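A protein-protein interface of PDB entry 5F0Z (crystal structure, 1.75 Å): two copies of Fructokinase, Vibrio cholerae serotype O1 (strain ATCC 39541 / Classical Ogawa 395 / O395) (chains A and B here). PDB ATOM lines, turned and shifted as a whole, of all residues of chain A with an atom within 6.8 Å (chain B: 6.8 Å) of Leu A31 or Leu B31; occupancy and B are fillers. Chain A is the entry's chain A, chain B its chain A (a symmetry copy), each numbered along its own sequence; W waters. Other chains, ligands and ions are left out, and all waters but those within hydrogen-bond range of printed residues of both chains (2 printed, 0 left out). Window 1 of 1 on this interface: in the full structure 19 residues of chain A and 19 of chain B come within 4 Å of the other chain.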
ATOM      1  N   VAL A  28     -21.012 -25.522   2.391  1.00  0.00           N
ATOM      2  CA  VAL A  28     -20.076 -25.442   1.288  1.00  0.00           C
ATOM      3  C   VAL A  28     -20.421 -24.222   0.440  1.00  0.00           C
ATOM      4  O   VAL A  28     -21.593 -23.875   0.303  1.00  0.00           O
ATOM      5  CB  VAL A  28     -20.322 -26.679   0.397  1.00  0.00           C
ATOM      6  CG1 VAL A  28     -19.681 -26.575  -0.935  1.00  0.00           C
ATOM      7  CG2 VAL A  28     -19.964 -27.966   1.160  1.00  0.00           C
ATOM      8  N   VAL A  29     -19.405 -23.598  -0.142  1.00  0.00           N
ATOM      9  CA  VAL A  29     -19.634 -22.686  -1.255  1.00  0.00           C
ATOM     10  C   VAL A  29     -19.525 -23.440  -2.576  1.00  0.00           C
ATOM     11  O   VAL A  29     -18.491 -24.034  -2.895  1.00  0.00           O
ATOM     12  CB  VAL A  29     -18.667 -21.479  -1.223  1.00  0.00           C
ATOM     13  CG1 VAL A  29     -18.782 -20.671  -2.501  1.00  0.00           C
ATOM     14  CG2 VAL A  29     -18.973 -20.611  -0.034  1.00  0.00           C
ATOM     15  N   ASP A  30     -20.617 -23.394  -3.343  1.00  0.00           N
ATOM     16  CA  ASP A  30     -20.669 -24.025  -4.641  1.00  0.00           C
ATOM     17  C   ASP A  30     -20.399 -22.922  -5.644  1.00  0.00           C
ATOM     18  O   ASP A  30     -21.120 -21.900  -5.673  1.00  0.00           O
ATOM     19  CB  ASP A  30     -22.061 -24.604  -4.941  1.00  0.00           C
ATOM     20  CG  ASP A  30     -22.368 -25.928  -4.214  1.00  0.00           C
ATOM     21  OD1 ASP A  30     -21.455 -26.700  -3.900  1.00  0.00           O
ATOM     22  OD2 ASP A  30     -23.562 -26.194  -4.004  1.00  0.00           O
ATOM     23  N   LEU A  31     -19.393 -23.132  -6.483  1.00  0.00           N
ATOM     24  CA  LEU A  31     -19.057 -22.190  -7.532  1.00  0.00           C
ATOM     25  C   LEU A  31     -19.683 -22.701  -8.802  1.00  0.00           C
ATOM     26  O   LEU A  31     -19.285 -23.716  -9.320  1.00  0.00           O
ATOM     27  CB  LEU A  31     -17.530 -22.070  -7.678  1.00  0.00           C
ATOM     28  CG  LEU A  31     -16.772 -21.594  -6.437  1.00  0.00           C
ATOM     29  CD1 LEU A  31     -15.302 -21.829  -6.609  1.00  0.00           C
ATOM     30  CD2 LEU A  31     -17.041 -20.116  -6.153  1.00  0.00           C
ATOM     31  N   ILE A  32     -20.684 -21.973  -9.294  1.00  0.00           N
ATOM     32  CA  ILE A  32     -21.505 -22.436 -10.394  1.00  0.00           C
ATOM     33  C   ILE A  32     -21.322 -21.519 -11.603  1.00  0.00           C
ATOM     34  O   ILE A  32     -21.517 -20.309 -11.520  1.00  0.00           O
ATOM     35  CB  ILE A  32     -22.996 -22.496  -9.952  1.00  0.00           C
ATOM     36  CG1 ILE A  32     -23.133 -23.446  -8.765  1.00  0.00           C
ATOM     37  CG2 ILE A  32     -23.865 -22.907 -11.113  1.00  0.00           C
ATOM     38  CD1 ILE A  32     -24.579 -23.641  -8.256  1.00  0.00           C
ATOM     39  N   PRO A  33     -20.908 -22.090 -12.739  1.00  0.00           N
ATOM     40  CA  PRO A  33     -20.687 -21.248 -13.913  1.00  0.00           C
ATOM     41  C   PRO A  33     -21.893 -20.388 -14.263  1.00  0.00           C
ATOM     42  O   PRO A  33     -23.026 -20.873 -14.179  1.00  0.00           O
ATOM     43  CB  PRO A  33     -20.444 -22.273 -15.010  1.00  0.00           C
ATOM     44  CG  PRO A  33     -19.813 -23.420 -14.289  1.00  0.00           C
ATOM     45  CD  PRO A  33     -20.522 -23.493 -12.984  1.00  0.00           C
ATOM     46  N   TYR A  39     -18.114 -17.312 -12.058  1.00  0.00           N
ATOM     47  CA  TYR A  39     -18.802 -18.248 -11.207  1.00  0.00           C
ATOM     48  C   TYR A  39     -19.766 -17.463 -10.346  1.00  0.00           C
ATOM     49  O   TYR A  39     -19.424 -16.401  -9.848  1.00  0.00           O
ATOM     50  CB  TYR A  39     -17.832 -18.950 -10.271  1.00  0.00           C
ATOM     51  CG  TYR A  39     -16.997 -20.022 -10.898  1.00  0.00           C
ATOM     52  CD1 TYR A  39     -17.578 -21.162 -11.449  1.00  0.00           C
ATOM     53  CD2 TYR A  39     -15.614 -19.918 -10.905  1.00  0.00           C
ATOM     54  CE1 TYR A  39     -16.800 -22.148 -12.027  1.00  0.00           C
ATOM     55  CE2 TYR A  39     -14.837 -20.897 -11.457  1.00  0.00           C
ATOM     56  CZ  TYR A  39     -15.432 -22.008 -12.018  1.00  0.00           C
ATOM     57  OH  TYR A  39     -14.629 -22.959 -12.587  1.00  0.00           O
ATOM     58  N   LEU A  40     -20.967 -17.999 -10.167  1.00  0.00           N
ATOM     59  CA  LEU A  40     -21.842 -17.575  -9.081  1.00  0.00           C
ATOM     60  C   LEU A  40     -21.290 -18.111  -7.770  1.00  0.00           C
ATOM     61  O   LEU A  40     -20.800 -19.235  -7.699  1.00  0.00           O
ATOM     62  CB  LEU A  40     -23.256 -18.114  -9.290  1.00  0.00           C
ATOM     63  CG  LEU A  40     -24.060 -17.456 -10.392  1.00  0.00           C
ATOM     64  CD1 LEU A  40     -25.284 -18.295 -10.713  1.00  0.00           C
ATOM     65  CD2 LEU A  40     -24.469 -16.060  -9.973  1.00  0.00           C
ATOM     66  N   LYS A  41     -21.344 -17.299  -6.730  1.00  0.00           N
ATOM     67  CA  LYS A  41     -20.955 -17.747  -5.393  1.00  0.00           C
ATOM     68  C   LYS A  41     -22.204 -18.169  -4.673  1.00  0.00           C
ATOM     69  O   LYS A  41     -22.911 -17.322  -4.112  1.00  0.00           O
ATOM     70  CB  LYS A  41     -20.320 -16.594  -4.644  1.00  0.00           C
ATOM     71  CG  LYS A  41     -19.788 -16.904  -3.273  1.00  0.00           C
ATOM     72  CD  LYS A  41     -19.592 -15.566  -2.615  1.00  0.00           C
ATOM     73  CE  LYS A  41     -18.934 -15.617  -1.281  1.00  0.00           C
ATOM     74  NZ  LYS A  41     -18.866 -14.212  -0.742  1.00  0.00           N
ATOM     75  N   CYS A  42     -22.490 -19.463  -4.711  1.00  0.00           N
ATOM     76  CA  CYS A  42     -23.740 -19.992  -4.196  1.00  0.00           C
ATOM     77  C   CYS A  42     -23.549 -20.766  -2.915  1.00  0.00           C
ATOM     78  O   CYS A  42     -22.736 -21.680  -2.823  1.00  0.00           O
ATOM     79  CB  CYS A  42     -24.446 -20.907  -5.206  1.00  0.00           C
ATOM     80  SG  CYS A  42     -24.803 -20.201  -6.814  1.00  0.00           S
ATOM     81  N   PHE A  72     -15.629 -17.664   3.304  1.00  0.00           N
ATOM     82  CA  PHE A  72     -16.640 -18.627   2.897  1.00  0.00           C
ATOM     83  C   PHE A  72     -17.397 -19.210   4.120  1.00  0.00           C
ATOM     84  O   PHE A  72     -18.634 -19.411   4.082  1.00  0.00           O
ATOM     85  CB  PHE A  72     -16.035 -19.758   2.061  1.00  0.00           C
ATOM     86  CG  PHE A  72     -15.727 -19.388   0.633  1.00  0.00           C
ATOM     87  CD1 PHE A  72     -15.908 -18.093   0.163  1.00  0.00           C
ATOM     88  CD2 PHE A  72     -15.244 -20.347  -0.240  1.00  0.00           C
ATOM     89  CE1 PHE A  72     -15.601 -17.771  -1.143  1.00  0.00           C
ATOM     90  CE2 PHE A  72     -14.927 -20.027  -1.546  1.00  0.00           C
ATOM     91  CZ  PHE A  72     -15.142 -18.730  -1.998  1.00  0.00           C
ATOM     92  N   THR A 100     -15.153 -25.981  -0.629  1.00  0.00           N
ATOM     93  CA  THR A 100     -15.330 -25.176  -1.827  1.00  0.00           C
ATOM     94  C   THR A 100     -15.439 -26.162  -2.958  1.00  0.00           C
ATOM     95  O   THR A 100     -14.532 -26.987  -3.164  1.00  0.00           O
ATOM     96  CB  THR A 100     -14.111 -24.250  -2.061  1.00  0.00           C
ATOM     97  OG1 THR A 100     -13.885 -23.451  -0.899  1.00  0.00           O
ATOM     98  CG2 THR A 100     -14.315 -23.346  -3.289  1.00  0.00           C
ATOM     99  N   VAL A 101     -16.552 -26.084  -3.682  1.00  0.00           N
ATOM    100  CA  VAL A 101     -16.900 -27.067  -4.711  1.00  0.00           C
ATOM    101  C   VAL A 101     -17.154 -26.382  -6.034  1.00  0.00           C
ATOM    102  O   VAL A 101     -17.829 -25.375  -6.078  1.00  0.00           O
ATOM    103  CB  VAL A 101     -18.181 -27.848  -4.303  1.00  0.00           C
ATOM    104  CG1 VAL A 101     -18.687 -28.718  -5.426  1.00  0.00           C
ATOM    105  CG2 VAL A 101     -17.934 -28.673  -3.060  1.00  0.00           C
ATOM    106  N   VAL A 102     -16.577 -26.916  -7.106  1.00  0.00           N
ATOM    107  CA  VAL A 102     -16.780 -26.375  -8.444  1.00  0.00           C
ATOM    108  C   VAL A 102     -17.782 -27.268  -9.165  1.00  0.00           C
ATOM    109  O   VAL A 102     -17.650 -28.489  -9.182  1.00  0.00           O
ATOM    110  CB  VAL A 102     -15.456 -26.313  -9.238  1.00  0.00           C
ATOM    111  CG1 VAL A 102     -15.658 -25.758 -10.659  1.00  0.00           C
ATOM    112  CG2 VAL A 102     -14.441 -25.446  -8.502  1.00  0.00           C
ATOM    113  N   VAL A 103     -18.810 -26.647  -9.743  1.00  0.00           N
ATOM    114  CA  VAL A 103     -19.898 -27.369 -10.381  1.00  0.00           C
ATOM    115  C   VAL A 103     -19.744 -27.325 -11.891  1.00  0.00           C
ATOM    116  O   VAL A 103     -19.413 -26.274 -12.476  1.00  0.00           O
ATOM    117  CB  VAL A 103     -21.279 -26.780  -9.980  1.00  0.00           C
ATOM    118  CG1 VAL A 103     -22.416 -27.535 -10.669  1.00  0.00           C
ATOM    119  CG2 VAL A 103     -21.453 -26.791  -8.485  1.00  0.00           C
ATOM    120  N   ASP A 104     -19.949 -28.472 -12.526  1.00  0.00           N
ATOM    121  CA  ASP A 104     -19.937 -28.552 -13.986  1.00  0.00           C
ATOM    122  C   ASP A 104     -21.370 -28.818 -14.390  1.00  0.00           C
ATOM    123  O   ASP A 104     -21.907 -29.867 -14.080  1.00  0.00           O
ATOM    124  CB  ASP A 104     -19.015 -29.682 -14.446  1.00  0.00           C
ATOM    125  CG  ASP A 104     -19.031 -29.892 -15.948  1.00  0.00           C
ATOM    126  OD1 ASP A 104     -18.145 -30.623 -16.453  1.00  0.00           O
ATOM    127  OD2 ASP A 104     -19.903 -29.327 -16.635  1.00  0.00           O
ATOM    128  N   MET A 116     -12.569 -28.960  -3.916  1.00  0.00           N
ATOM    129  CA  MET A 116     -11.229 -28.367  -3.894  1.00  0.00           C
ATOM    130  C   MET A 116     -10.556 -28.426  -2.527  1.00  0.00           C
ATOM    131  O   MET A 116      -9.319 -28.369  -2.432  1.00  0.00           O
ATOM    132  CB  MET A 116     -11.266 -26.927  -4.382  1.00  0.00           C
ATOM    133  CG  MET A 116     -11.745 -26.785  -5.800  1.00  0.00           C
ATOM    134  SD  MET A 116     -10.844 -27.763  -6.984  1.00  0.00           S
ATOM    135  CE  MET A 116      -9.240 -26.955  -6.889  1.00  0.00           C
ATOM    136  N   VAL B  28      -2.265 -20.855  -9.779  1.00  0.00           N
ATOM    137  CA  VAL B  28      -3.403 -20.698  -8.895  1.00  0.00           C
ATOM    138  C   VAL B  28      -4.573 -20.138  -9.699  1.00  0.00           C
ATOM    139  O   VAL B  28      -4.370 -19.346 -10.617  1.00  0.00           O
ATOM    140  CB  VAL B  28      -3.025 -19.617  -7.860  1.00  0.00           C
ATOM    141  CG1 VAL B  28      -4.188 -19.107  -7.097  1.00  0.00           C
ATOM    142  CG2 VAL B  28      -1.868 -20.110  -6.973  1.00  0.00           C
ATOM    143  N   VAL B  29      -5.786 -20.530  -9.331  1.00  0.00           N
ATOM    144  CA  VAL B  29      -6.966 -19.787  -9.753  1.00  0.00           C
ATOM    145  C   VAL B  29      -7.324 -18.740  -8.704  1.00  0.00           C
ATOM    146  O   VAL B  29      -7.582 -19.058  -7.539  1.00  0.00           O
ATOM    147  CB  VAL B  29      -8.166 -20.719 -10.040  1.00  0.00           C
ATOM    148  CG1 VAL B  29      -9.428 -19.908 -10.262  1.00  0.00           C
ATOM    149  CG2 VAL B  29      -7.877 -21.568 -11.248  1.00  0.00           C
ATOM    150  N   ASP B  30      -7.342 -17.481  -9.147  1.00  0.00           N
ATOM    151  CA  ASP B  30      -7.696 -16.372  -8.291  1.00  0.00           C
ATOM    152  C   ASP B  30      -9.154 -16.079  -8.582  1.00  0.00           C
ATOM    153  O   ASP B  30      -9.528 -15.815  -9.747  1.00  0.00           O
ATOM    154  CB  ASP B  30      -6.887 -15.109  -8.625  1.00  0.00           C
ATOM    155  CG  ASP B  30      -5.435 -15.130  -8.106  1.00  0.00           C
ATOM    156  OD1 ASP B  30      -5.137 -15.782  -7.099  1.00  0.00           O
ATOM    157  OD2 ASP B  30      -4.608 -14.434  -8.715  1.00  0.00           O
ATOM    158  N   LEU B  31      -9.971 -16.092  -7.537  1.00  0.00           N
ATOM    159  CA  LEU B  31     -11.379 -15.774  -7.657  1.00  0.00           C
ATOM    160  C   LEU B  31     -11.543 -14.334  -7.247  1.00  0.00           C
ATOM    161  O   LEU B  31     -11.366 -13.995  -6.103  1.00  0.00           O
ATOM    162  CB  LEU B  31     -12.219 -16.701  -6.762  1.00  0.00           C
ATOM    163  CG  LEU B  31     -12.107 -18.199  -7.056  1.00  0.00           C
ATOM    164  CD1 LEU B  31     -12.704 -18.990  -5.932  1.00  0.00           C
ATOM    165  CD2 LEU B  31     -12.790 -18.560  -8.376  1.00  0.00           C
ATOM    166  N   ILE B  32     -11.883 -13.486  -8.217  1.00  0.00           N
ATOM    167  CA  ILE B  32     -11.889 -12.051  -8.018  1.00  0.00           C
ATOM    168  C   ILE B  32     -13.312 -11.511  -8.160  1.00  0.00           C
ATOM    169  O   ILE B  32     -13.972 -11.716  -9.175  1.00  0.00           O
ATOM    170  CB  ILE B  32     -10.924 -11.373  -9.033  1.00  0.00           C
ATOM    171  CG1 ILE B  32      -9.514 -11.920  -8.832  1.00  0.00           C
ATOM    172  CG2 ILE B  32     -10.980  -9.874  -8.881  1.00  0.00           C
ATOM    173  CD1 ILE B  32      -8.438 -11.289  -9.746  1.00  0.00           C
ATOM    174  N   PRO B  33     -13.811 -10.839  -7.118  1.00  0.00           N
ATOM    175  CA  PRO B  33     -15.180 -10.333  -7.194  1.00  0.00           C
ATOM    176  C   PRO B  33     -15.430  -9.482  -8.430  1.00  0.00           C
ATOM    177  O   PRO B  33     -14.561  -8.685  -8.802  1.00  0.00           O
ATOM    178  CB  PRO B  33     -15.282  -9.474  -5.943  1.00  0.00           C
ATOM    179  CG  PRO B  33     -14.364 -10.148  -4.976  1.00  0.00           C
ATOM    180  CD  PRO B  33     -13.207 -10.601  -5.792  1.00  0.00           C
ATOM    181  N   TYR B  39     -17.771 -14.248  -9.068  1.00  0.00           N
ATOM    182  CA  TYR B  39     -16.333 -14.194  -9.101  1.00  0.00           C
ATOM    183  C   TYR B  39     -15.900 -14.354 -10.542  1.00  0.00           C
ATOM    184  O   TYR B  39     -16.445 -15.177 -11.261  1.00  0.00           O
ATOM    185  CB  TYR B  39     -15.725 -15.346  -8.318  1.00  0.00           C
ATOM    186  CG  TYR B  39     -15.768 -15.204  -6.829  1.00  0.00           C
ATOM    187  CD1 TYR B  39     -15.098 -14.169  -6.181  1.00  0.00           C
ATOM    188  CD2 TYR B  39     -16.449 -16.133  -6.057  1.00  0.00           C
ATOM    189  CE1 TYR B  39     -15.144 -14.043  -4.805  1.00  0.00           C
ATOM    190  CE2 TYR B  39     -16.483 -16.028  -4.695  1.00  0.00           C
ATOM    191  CZ  TYR B  39     -15.832 -14.983  -4.073  1.00  0.00           C
ATOM    192  OH  TYR B  39     -15.906 -14.888  -2.710  1.00  0.00           O
ATOM    193  N   LEU B  40     -14.909 -13.570 -10.950  1.00  0.00           N
ATOM    194  CA  LEU B  40     -14.140 -13.870 -12.152  1.00  0.00           C
ATOM    195  C   LEU B  40     -13.230 -15.053 -11.869  1.00  0.00           C
ATOM    196  O   LEU B  40     -12.662 -15.173 -10.786  1.00  0.00           O
ATOM    197  CB  LEU B  40     -13.292 -12.666 -12.558  1.00  0.00           C
ATOM    198  CG  LEU B  40     -14.045 -11.495 -13.154  1.00  0.00           C
ATOM    199  CD1 LEU B  40     -13.150 -10.268 -13.191  1.00  0.00           C
ATOM    200  CD2 LEU B  40     -14.529 -11.842 -14.546  1.00  0.00           C
ATOM    201  N   LYS B  41     -13.105 -15.947 -12.832  1.00  0.00           N
ATOM    202  CA  LYS B  41     -12.165 -17.063 -12.720  1.00  0.00           C
ATOM    203  C   LYS B  41     -10.899 -16.661 -13.421  1.00  0.00           C
ATOM    204  O   LYS B  41     -10.803 -16.790 -14.649  1.00  0.00           O
ATOM    205  CB  LYS B  41     -12.747 -18.278 -13.411  1.00  0.00           C
ATOM    206  CG  LYS B  41     -11.939 -19.543 -13.322  1.00  0.00           C
ATOM    207  CD  LYS B  41     -12.504 -20.447 -14.383  1.00  0.00           C
ATOM    208  CE  LYS B  41     -11.945 -21.826 -14.391  1.00  0.00           C
ATOM    209  NZ  LYS B  41     -12.571 -22.575 -15.538  1.00  0.00           N
ATOM    210  N   CYS B  42      -9.943 -16.153 -12.655  1.00  0.00           N
ATOM    211  CA  CYS B  42      -8.732 -15.579 -13.211  1.00  0.00           C
ATOM    212  C   CYS B  42      -7.523 -16.450 -12.967  1.00  0.00           C
ATOM    213  O   CYS B  42      -7.222 -16.845 -11.845  1.00  0.00           O
ATOM    214  CB  CYS B  42      -8.435 -14.184 -12.647  1.00  0.00           C
ATOM    215  SG  CYS B  42      -9.725 -12.954 -12.834  1.00  0.00           S
ATOM    216  N   PHE B  72      -9.250 -26.831 -12.437  1.00  0.00           N
ATOM    217  CA  PHE B  72      -8.420 -25.655 -12.227  1.00  0.00           C
ATOM    218  C   PHE B  72      -6.957 -25.903 -12.680  1.00  0.00           C
ATOM    219  O   PHE B  72      -6.304 -25.016 -13.278  1.00  0.00           O
ATOM    220  CB  PHE B  72      -8.451 -25.198 -10.766  1.00  0.00           C
ATOM    221  CG  PHE B  72      -9.702 -24.460 -10.366  1.00  0.00           C
ATOM    222  CD1 PHE B  72     -10.763 -24.296 -11.249  1.00  0.00           C
ATOM    223  CD2 PHE B  72      -9.816 -23.935  -9.091  1.00  0.00           C
ATOM    224  CE1 PHE B  72     -11.907 -23.633 -10.855  1.00  0.00           C
ATOM    225  CE2 PHE B  72     -10.964 -23.278  -8.690  1.00  0.00           C
ATOM    226  CZ  PHE B  72     -12.000 -23.105  -9.601  1.00  0.00           C
ATOM    227  N   THR B 100      -6.383 -22.443  -4.861  1.00  0.00           N
ATOM    228  CA  THR B 100      -7.567 -21.649  -5.146  1.00  0.00           C
ATOM    229  C   THR B 100      -7.560 -20.542  -4.126  1.00  0.00           C
ATOM    230  O   THR B 100      -7.541 -20.805  -2.912  1.00  0.00           O
ATOM    231  CB  THR B 100      -8.856 -22.493  -4.988  1.00  0.00           C
ATOM    232  OG1 THR B 100      -8.772 -23.656  -5.812  1.00  0.00           O
ATOM    233  CG2 THR B 100     -10.111 -21.681  -5.351  1.00  0.00           C
ATOM    234  N   VAL B 101      -7.565 -19.307  -4.620  1.00  0.00           N
ATOM    235  CA  VAL B 101      -7.392 -18.118  -3.783  1.00  0.00           C
ATOM    236  C   VAL B 101      -8.540 -17.155  -3.987  1.00  0.00           C
ATOM    237  O   VAL B 101      -8.933 -16.906  -5.107  1.00  0.00           O
ATOM    238  CB  VAL B 101      -6.066 -17.390  -4.141  1.00  0.00           C
ATOM    239  CG1 VAL B 101      -5.956 -16.055  -3.450  1.00  0.00           C
ATOM    240  CG2 VAL B 101      -4.872 -18.258  -3.814  1.00  0.00           C
ATOM    241  N   VAL B 102      -9.097 -16.645  -2.893  1.00  0.00           N
ATOM    242  CA  VAL B 102     -10.180 -15.673  -2.957  1.00  0.00           C
ATOM    243  C   VAL B 102      -9.593 -14.294  -2.687  1.00  0.00           C
ATOM    244  O   VAL B 102      -8.856 -14.093  -1.725  1.00  0.00           O
ATOM    245  CB  VAL B 102     -11.289 -15.990  -1.928  1.00  0.00           C
ATOM    246  CG1 VAL B 102     -12.433 -14.962  -1.974  1.00  0.00           C
ATOM    247  CG2 VAL B 102     -11.856 -17.382  -2.176  1.00  0.00           C
ATOM    248  N   VAL B 103      -9.903 -13.342  -3.567  1.00  0.00           N
ATOM    249  CA  VAL B 103      -9.338 -12.005  -3.500  1.00  0.00           C
ATOM    250  C   VAL B 103     -10.357 -11.032  -2.933  1.00  0.00           C
ATOM    251  O   VAL B 103     -11.552 -11.068  -3.290  1.00  0.00           O
ATOM    252  CB  VAL B 103      -8.874 -11.516  -4.901  1.00  0.00           C
ATOM    253  CG1 VAL B 103      -8.298 -10.102  -4.823  1.00  0.00           C
ATOM    254  CG2 VAL B 103      -7.877 -12.472  -5.500  1.00  0.00           C
ATOM    255  N   ASP B 104      -9.900 -10.183  -2.022  1.00  0.00           N
ATOM    256  CA  ASP B 104     -10.743  -9.125  -1.470  1.00  0.00           C
ATOM    257  C   ASP B 104     -10.185  -7.830  -2.018  1.00  0.00           C
ATOM    258  O   ASP B 104      -9.069  -7.463  -1.697  1.00  0.00           O
ATOM    259  CB  ASP B 104     -10.685  -9.146   0.059  1.00  0.00           C
ATOM    260  CG  ASP B 104     -11.458  -8.010   0.702  1.00  0.00           C
ATOM    261  OD1 ASP B 104     -11.674  -8.066   1.937  1.00  0.00           O
ATOM    262  OD2 ASP B 104     -11.866  -7.071  -0.006  1.00  0.00           O
ATOM    263  N   MET B 116      -7.564 -21.113  -0.045  1.00  0.00           N
ATOM    264  CA  MET B 116      -8.530 -22.145   0.340  1.00  0.00           C
ATOM    265  C   MET B 116      -7.952 -23.556   0.336  1.00  0.00           C
ATOM    266  O   MET B 116      -8.475 -24.452   1.019  1.00  0.00           O
ATOM    267  CB  MET B 116      -9.760 -22.096  -0.553  1.00  0.00           C
ATOM    268  CG  MET B 116     -10.509 -20.794  -0.473  1.00  0.00           C
ATOM    269  SD  MET B 116     -10.984 -20.318   1.175  1.00  0.00           S
ATOM    270  CE  MET B 116     -12.164 -21.625   1.544  1.00  0.00           C
HETATM  271  O   HOH W   1     -10.995 -27.678 -10.233  1.00  0.00           O
HETATM  272  O   HOH W   2     -12.958 -17.905   2.109  1.00  0.00           O
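Hydrophobic or aromatic side chains of chain A within 4 Å of the printed part of chain B: Leu A31, Tyr A39, Phe A72, Val A102 and Met A116. Along chain A the printed residues that touch a printed residue of chain B span positions 31 to 116. Hydrophobic or aromatic side chains of chain B within 4 Å of the printed part of chain A: Leu B31, Tyr B39, Phe B72, Val B102 and Met B116. Among the printed residues, 12 pairs touch across the chains. Among the printed residues, no Asp or Glu carboxylate lies within 4 Å of a Lys or Arg side-chain nitrogen of the other chain.
The backbone NH of Val A103 sits at hydrogen-bond distance from the backbone carbonyl oxygen of Leu A31 (3.0 Å). The backbone NH (N) of Leu B31 lies within hydrogen-bond range of the backbone carbonyl oxygen (O) of Val B101 (2.8 Å). The backbone carbonyl oxygen (O) of Leu B31 sits at hydrogen-bond distance from the backbone NH (N) of Val B103. The backbone NH (N) of Met A116 sits at hydrogen-bond distance from the backbone carbonyl oxygen (O) of Thr A100 (2.9 Å). N of Leu A31 is in hydrogen-bond range of O of Val A101. O of Thr B100 lies within hydrogen-bond range of N of Met B116 (2.9 Å).
Tyr A39 touches Phe B72, and with the chains exchanged Phe A72 touches Tyr B39. Phe A72 touches Val B102, and with the chains exchanged Val A102 touches Phe B72. Phe A72 touches Met B116, and with the chains exchanged Met A116 touches Phe B72. Thr A100 touches Met B116, and with the chains exchanged Met A116 touches Thr B100. Of the 12 pairs that touch across the chains among the printed residues, 12 have their exchanged pair printed and touching as well.
Printed residues of chain B within 4 Å of Leu A31: Leu B31. Of chain A, only Leu A31 comes within 4 Å of Leu B31. Of the printed residues of chain B, Lys A41 touches Tyr B39. Printed residues of chain B within 4 Å of Tyr A39: Tyr B39, Lys B41 and Phe B72. Printed residues of chain B within 4 Å of Val A102: Phe B72. Of the printed residues of chain A, Val B102 touches Phe A72. Printed residues of chain A within 4 Å of Met B116: Phe A72 and Thr A100. Asp A104 touches none of the printed residues of chain B. Pro B33 touches none of the printed residues of chain A. The nearest residue of chain B that does not touch Leu A31 is Tyr B39 (4.03 Å). The nearest residue of chain A that does not touch Leu B31 is Tyr A39 (4.03 Å).
Among the printed residues, pairs that only touch across the chains: Phe A72 with Tyr B39 (3.3 Å), Tyr A39 with Phe B72 (3.3 Å), Tyr A39 with Lys B41 (3.4 Å), Lys A41 with Tyr B39 (3.4 Å), Met A116 with Thr B100 (3.5 Å), Thr A100 with Met B116 (3.5 Å), Val A102 with Phe B72 (3.6 Å), Phe A72 with Val B102 (3.6 Å), Met A116 with Phe B72 (3.8 Å), Phe A72 with Met B116 (3.8 Å) and Leu A31 with Leu B31 (3.9 Å).
The backbone NH (N) of Tyr A39 sits at hydrogen-bond distance from the backbone carbonyl oxygen (O) of Tyr B39, at 2.8 Å.
Water W2 bridges the backbone NH (N) of Phe A72 and the side-chain sulfur (SD) of Met B116. Water W1 bridges the backbone NH of Phe B72 (2.9 Å) and the side-chain sulfur of Met A116 (3.3 Å).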
